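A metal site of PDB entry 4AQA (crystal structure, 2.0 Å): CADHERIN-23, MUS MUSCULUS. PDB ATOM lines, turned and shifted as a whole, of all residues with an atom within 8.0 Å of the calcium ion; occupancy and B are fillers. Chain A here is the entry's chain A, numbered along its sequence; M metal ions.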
ATOM      1  N   VAL A   3      -4.630 -19.990  -4.601  1.00  0.00           N
ATOM      2  CA  VAL A   3      -5.427 -18.767  -4.699  1.00  0.00           C
ATOM      3  C   VAL A   3      -4.481 -17.567  -4.821  1.00  0.00           C
ATOM      4  O   VAL A   3      -3.349 -17.605  -4.325  1.00  0.00           O
ATOM      5  CB  VAL A   3      -6.401 -18.558  -3.513  1.00  0.00           C
ATOM      6  CG1 VAL A   3      -7.353 -19.755  -3.369  1.00  0.00           C
ATOM      7  CG2 VAL A   3      -5.643 -18.297  -2.227  1.00  0.00           C
ATOM      8  N   ASN A   4      -4.932 -16.515  -5.491  1.00  0.00           N
ATOM      9  CA  ASN A   4      -4.126 -15.302  -5.631  1.00  0.00           C
ATOM     10  C   ASN A   4      -3.809 -14.700  -4.269  1.00  0.00           C
ATOM     11  O   ASN A   4      -4.662 -14.669  -3.394  1.00  0.00           O
ATOM     12  CB  ASN A   4      -4.827 -14.253  -6.478  1.00  0.00           C
ATOM     13  CG  ASN A   4      -4.017 -12.977  -6.598  1.00  0.00           C
ATOM     14  OD1 ASN A   4      -2.854 -13.005  -6.966  1.00  0.00           O
ATOM     15  ND2 ASN A   4      -4.622 -11.847  -6.253  1.00  0.00           N
ATOM     16  N   ARG A   5      -2.579 -14.250  -4.099  1.00  0.00           N
ATOM     17  CA  ARG A   5      -2.177 -13.484  -2.934  1.00  0.00           C
ATOM     18  C   ARG A   5      -1.965 -12.065  -3.386  1.00  0.00           C
ATOM     19  O   ARG A   5      -1.303 -11.808  -4.390  1.00  0.00           O
ATOM     20  CB  ARG A   5      -0.941 -14.120  -2.306  1.00  0.00           C
ATOM     21  CG  ARG A   5      -1.307 -15.459  -1.674  1.00  0.00           C
ATOM     22  CD  ARG A   5      -0.178 -16.463  -1.649  1.00  0.00           C
ATOM     23  NE  ARG A   5       0.327 -16.844  -2.958  1.00  0.00           N
ATOM     24  CZ  ARG A   5       1.503 -17.453  -3.142  1.00  0.00           C
ATOM     25  NH1 ARG A   5       2.275 -17.769  -2.104  1.00  0.00           N
ATOM     26  NH2 ARG A   5       1.917 -17.762  -4.365  1.00  0.00           N
ATOM     27  N   LEU A   6      -2.598 -11.158  -2.660  1.00  0.00           N
ATOM     28  CA  LEU A   6      -2.553  -9.743  -2.994  1.00  0.00           C
ATOM     29  C   LEU A   6      -1.161  -9.160  -2.705  1.00  0.00           C
ATOM     30  O   LEU A   6      -0.421  -9.641  -1.838  1.00  0.00           O
ATOM     31  CB  LEU A   6      -3.631  -8.978  -2.215  1.00  0.00           C
ATOM     32  CG  LEU A   6      -5.112  -9.343  -2.514  1.00  0.00           C
ATOM     33  CD1 LEU A   6      -6.074  -8.777  -1.486  1.00  0.00           C
ATOM     34  CD2 LEU A   6      -5.503  -8.914  -3.927  1.00  0.00           C
ATOM     35  N   PRO A   7      -0.786  -8.098  -3.443  1.00  0.00           N
ATOM     36  CA  PRO A   7       0.502  -7.473  -3.152  1.00  0.00           C
ATOM     37  C   PRO A   7       0.495  -6.689  -1.855  1.00  0.00           C
ATOM     38  O   PRO A   7      -0.575  -6.400  -1.326  1.00  0.00           O
ATOM     39  CB  PRO A   7       0.701  -6.519  -4.335  1.00  0.00           C
ATOM     40  CG  PRO A   7      -0.671  -6.244  -4.844  1.00  0.00           C
ATOM     41  CD  PRO A   7      -1.412  -7.546  -4.654  1.00  0.00           C
ATOM     42  N   PHE A   8       1.686  -6.331  -1.391  1.00  0.00           N
ATOM     43  CA  PHE A   8       1.875  -5.489  -0.193  1.00  0.00           C
ATOM     44  C   PHE A   8       3.040  -4.520  -0.395  1.00  0.00           C
ATOM     45  O   PHE A   8       4.034  -4.837  -1.048  1.00  0.00           O
ATOM     46  CB  PHE A   8       2.043  -6.350   1.082  1.00  0.00           C
ATOM     47  CG  PHE A   8       3.162  -7.354   1.002  1.00  0.00           C
ATOM     48  CD1 PHE A   8       2.931  -8.638   0.524  1.00  0.00           C
ATOM     49  CD2 PHE A   8       4.445  -7.013   1.442  1.00  0.00           C
ATOM     50  CE1 PHE A   8       3.964  -9.573   0.465  1.00  0.00           C
ATOM     51  CE2 PHE A   8       5.471  -7.946   1.376  1.00  0.00           C
ATOM     52  CZ  PHE A   8       5.237  -9.217   0.905  1.00  0.00           C
ATOM     53  N   ARG A  36       5.769  -6.043  -3.117  1.00  0.00           N
ATOM     54  CA  ARG A  36       6.061  -7.443  -3.368  1.00  0.00           C
ATOM     55  C   ARG A  36       4.751  -8.205  -3.542  1.00  0.00           C
ATOM     56  O   ARG A  36       3.685  -7.770  -3.081  1.00  0.00           O
ATOM     57  CB  ARG A  36       6.874  -8.040  -2.211  1.00  0.00           C
ATOM     58  CG  ARG A  36       8.226  -7.346  -1.987  1.00  0.00           C
ATOM     59  CD  ARG A  36       9.235  -7.738  -3.056  1.00  0.00           C
ATOM     60  NE  ARG A  36       9.546  -9.165  -2.974  1.00  0.00           N
ATOM     61  CZ  ARG A  36      10.507  -9.771  -3.654  1.00  0.00           C
ATOM     62  NH1 ARG A  36      11.243  -9.074  -4.501  1.00  0.00           N
ATOM     63  NH2 ARG A  36      10.709 -11.076  -3.493  1.00  0.00           N
ATOM     64  N   ASP A  37       4.861  -9.333  -4.253  1.00  0.00           N
ATOM     65  CA  ASP A  37       3.730 -10.214  -4.515  1.00  0.00           C
ATOM     66  C   ASP A  37       4.229 -11.644  -4.488  1.00  0.00           C
ATOM     67  O   ASP A  37       5.132 -12.013  -5.229  1.00  0.00           O
ATOM     68  CB  ASP A  37       3.110  -9.864  -5.863  1.00  0.00           C
ATOM     69  CG  ASP A  37       1.822 -10.606  -6.123  1.00  0.00           C
ATOM     70  OD1 ASP A  37       1.854 -11.816  -6.413  1.00  0.00           O
ATOM     71  OD2 ASP A  37       0.760  -9.971  -6.056  1.00  0.00           O
ATOM     72  N   MET A  38       3.628 -12.460  -3.643  1.00  0.00           N
ATOM     73  CA  MET A  38       4.082 -13.856  -3.502  1.00  0.00           C
ATOM     74  C   MET A  38       3.891 -14.699  -4.756  1.00  0.00           C
ATOM     75  O   MET A  38       4.496 -15.766  -4.862  1.00  0.00           O
ATOM     76  CB  MET A  38       3.370 -14.529  -2.338  1.00  0.00           C
ATOM     77  CG  MET A  38       3.701 -13.932  -0.976  1.00  0.00           C
ATOM     78  SD  MET A  38       5.473 -13.867  -0.622  1.00  0.00           S
ATOM     79  CE  MET A  38       5.898 -12.201  -1.108  1.00  0.00           C
ATOM     80  N   ASP A  39       3.056 -14.225  -5.690  1.00  0.00           N
ATOM     81  CA  ASP A  39       2.877 -14.903  -6.984  1.00  0.00           C
ATOM     82  C   ASP A  39       3.826 -14.386  -8.045  1.00  0.00           C
ATOM     83  O   ASP A  39       3.806 -14.830  -9.180  1.00  0.00           O
ATOM     84  CB  ASP A  39       1.431 -14.738  -7.488  1.00  0.00           C
ATOM     85  CG  ASP A  39       0.412 -15.012  -6.431  1.00  0.00           C
ATOM     86  OD1 ASP A  39       0.284 -16.185  -6.016  1.00  0.00           O
ATOM     87  OD2 ASP A  39      -0.295 -14.064  -6.007  1.00  0.00           O
ATOM     88  N   ASN A  40       4.660 -13.413  -7.678  1.00  0.00           N
ATOM     89  CA  ASN A  40       5.563 -12.754  -8.600  1.00  0.00           C
ATOM     90  C   ASN A  40       4.848 -11.990  -9.707  1.00  0.00           C
ATOM     91  O   ASN A  40       5.407 -11.758 -10.778  1.00  0.00           O
ATOM     92  CB  ASN A  40       6.608 -13.745  -9.138  1.00  0.00           C
ATOM     93  CG  ASN A  40       7.754 -13.943  -8.164  1.00  0.00           C
ATOM     94  OD1 ASN A  40       8.293 -12.975  -7.625  1.00  0.00           O
ATOM     95  ND2 ASN A  40       8.141 -15.169  -7.941  1.00  0.00           N
ATOM     96  N   ASP A  41       3.631 -11.564  -9.404  1.00  0.00           N
ATOM     97  CA  ASP A  41       2.796 -10.843 -10.351  1.00  0.00           C
ATOM     98  C   ASP A  41       3.411  -9.473 -10.652  1.00  0.00           C
ATOM     99  O   ASP A  41       3.917  -8.812  -9.742  1.00  0.00           O
ATOM    100  CB  ASP A  41       1.388 -10.621  -9.775  1.00  0.00           C
ATOM    101  CG  ASP A  41       0.577 -11.898  -9.669  1.00  0.00           C
ATOM    102  OD1 ASP A  41       0.868 -12.841 -10.419  1.00  0.00           O
ATOM    103  OD2 ASP A  41      -0.348 -11.948  -8.839  1.00  0.00           O
ATOM    104  N   PRO A  42       3.347  -9.052 -11.927  1.00  0.00           N
ATOM    105  CA  PRO A  42       3.747  -7.684 -12.277  1.00  0.00           C
ATOM    106  C   PRO A  42       2.761  -6.681 -11.663  1.00  0.00           C
ATOM    107  O   PRO A  42       1.535  -6.922 -11.675  1.00  0.00           O
ATOM    108  CB  PRO A  42       3.731  -7.680 -13.805  1.00  0.00           C
ATOM    109  CG  PRO A  42       2.969  -8.867 -14.234  1.00  0.00           C
ATOM    110  CD  PRO A  42       2.921  -9.841 -13.090  1.00  0.00           C
ATOM    111  N   LEU A  43       3.269  -5.623 -11.046  1.00  0.00           N
ATOM    112  CA  LEU A  43       2.434  -4.729 -10.257  1.00  0.00           C
ATOM    113  C   LEU A  43       2.222  -3.385 -10.942  1.00  0.00           C
ATOM    114  O   LEU A  43       3.105  -2.860 -11.619  1.00  0.00           O
ATOM    115  CB  LEU A  43       3.025  -4.548  -8.850  1.00  0.00           C
ATOM    116  CG  LEU A  43       3.248  -5.870  -8.067  1.00  0.00           C
ATOM    117  CD1 LEU A  43       3.800  -5.652  -6.668  1.00  0.00           C
ATOM    118  CD2 LEU A  43       1.961  -6.665  -7.987  1.00  0.00           C
ATOM    119  N   SER A  86      -1.599  -2.926  -7.444  1.00  0.00           N
ATOM    120  CA  SER A  86      -2.530  -3.940  -7.964  1.00  0.00           C
ATOM    121  C   SER A  86      -1.770  -4.986  -8.719  1.00  0.00           C
ATOM    122  O   SER A  86      -0.847  -4.662  -9.449  1.00  0.00           O
ATOM    123  CB  SER A  86      -3.551  -3.284  -8.896  1.00  0.00           C
ATOM    124  OG  SER A  86      -4.298  -4.250  -9.606  1.00  0.00           O
ATOM    125  N   ASP A  87      -2.164  -6.255  -8.541  1.00  0.00           N
ATOM    126  CA  ASP A  87      -1.649  -7.356  -9.351  1.00  0.00           C
ATOM    127  C   ASP A  87      -2.641  -7.753 -10.470  1.00  0.00           C
ATOM    128  O   ASP A  87      -2.593  -8.858 -10.954  1.00  0.00           O
ATOM    129  CB  ASP A  87      -1.320  -8.555  -8.454  1.00  0.00           C
ATOM    130  CG  ASP A  87      -2.550  -9.145  -7.764  1.00  0.00           C
ATOM    131  OD1 ASP A  87      -3.677  -8.601  -7.941  1.00  0.00           O
ATOM    132  OD2 ASP A  87      -2.387 -10.142  -7.009  1.00  0.00           O
ATOM    133  N   HIS A  88      -3.527  -6.828 -10.862  1.00  0.00           N
ATOM    134  CA  HIS A  88      -4.602  -7.059 -11.856  1.00  0.00           C
ATOM    135  C   HIS A  88      -5.702  -7.979 -11.382  1.00  0.00           C
ATOM    136  O   HIS A  88      -6.620  -8.285 -12.152  1.00  0.00           O
ATOM    137  CB  HIS A  88      -4.056  -7.565 -13.191  1.00  0.00           C
ATOM    138  CG  HIS A  88      -2.981  -6.682 -13.784  1.00  0.00           C
ATOM    139  ND1 HIS A  88      -1.748  -7.146 -14.073  1.00  0.00           N
ATOM    140  CD2 HIS A  88      -2.993  -5.332 -14.142  1.00  0.00           C
ATOM    141  CE1 HIS A  88      -1.006  -6.148 -14.602  1.00  0.00           C
ATOM    142  NE2 HIS A  88      -1.763  -5.036 -14.634  1.00  0.00           N
ATOM    143  N   GLN A  89      -5.642  -8.442 -10.134  1.00  0.00           N
ATOM    144  CA  GLN A  89      -6.722  -9.259  -9.570  1.00  0.00           C
ATOM    145  C   GLN A  89      -7.382  -8.594  -8.413  1.00  0.00           C
ATOM    146  O   GLN A  89      -8.533  -8.854  -8.116  1.00  0.00           O
ATOM    147  CB  GLN A  89      -6.211 -10.625  -9.156  1.00  0.00           C
ATOM    148  CG  GLN A  89      -6.040 -11.557 -10.335  1.00  0.00           C
ATOM    149  CD  GLN A  89      -5.789 -12.980  -9.904  1.00  0.00           C
ATOM    150  OE1 GLN A  89      -6.706 -13.671  -9.427  1.00  0.00           O
ATOM    151  NE2 GLN A  89      -4.544 -13.421 -10.052  1.00  0.00           N
ATOM    152  N   GLY A  90      -6.631  -7.749  -7.721  1.00  0.00           N
ATOM    153  CA  GLY A  90      -7.188  -6.957  -6.648  1.00  0.00           C
ATOM    154  C   GLY A  90      -6.279  -5.772  -6.436  1.00  0.00           C
ATOM    155  O   GLY A  90      -5.104  -5.807  -6.833  1.00  0.00           O
HETATM  156 CA    CA M   1      -0.799 -11.803  -6.614  1.00  0.00          CA
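Within 4 Å of the calcium ion: Asn 4, Arg 5, Asp 37, Asp 39, Asp 41 and Asp 87. Along chain A the residues within 4 Å of the calcium ion span positions 4 to 87.
O of Met 38 is in hydrogen-bond range of NH2 of Arg 5, 3.3 Å away. OD1 of Asp 87 sits at hydrogen-bond distance from N of Gln 89, at 2.9 Å. The side-chain carboxylate of Asp 87 lies within hydrogen-bond range of the backbone NH of Gly 90, at 3.1 Å. OD1 of Asp 37 lies close to N of Asn 40.
The calcium ion is bound by the side-chain carboxylate (OD2) of Asp 41 (2.3 Å), the backbone carbonyl oxygen (O) of Arg 5 (2.3 Å), the side-chain carboxylate (OD2) of Asp 87 (2.3 Å), the side-chain carboxylate (OD2) of Asp 39 (2.4 Å), the side-chain amide oxygen (OD1) of Asn 4 (2.4 Å), the side-chain carboxylate (OD2) of Asp 37 (2.5 Å) and the side-chain carboxylate (OD1) of Asp 37 (2.7 Å).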
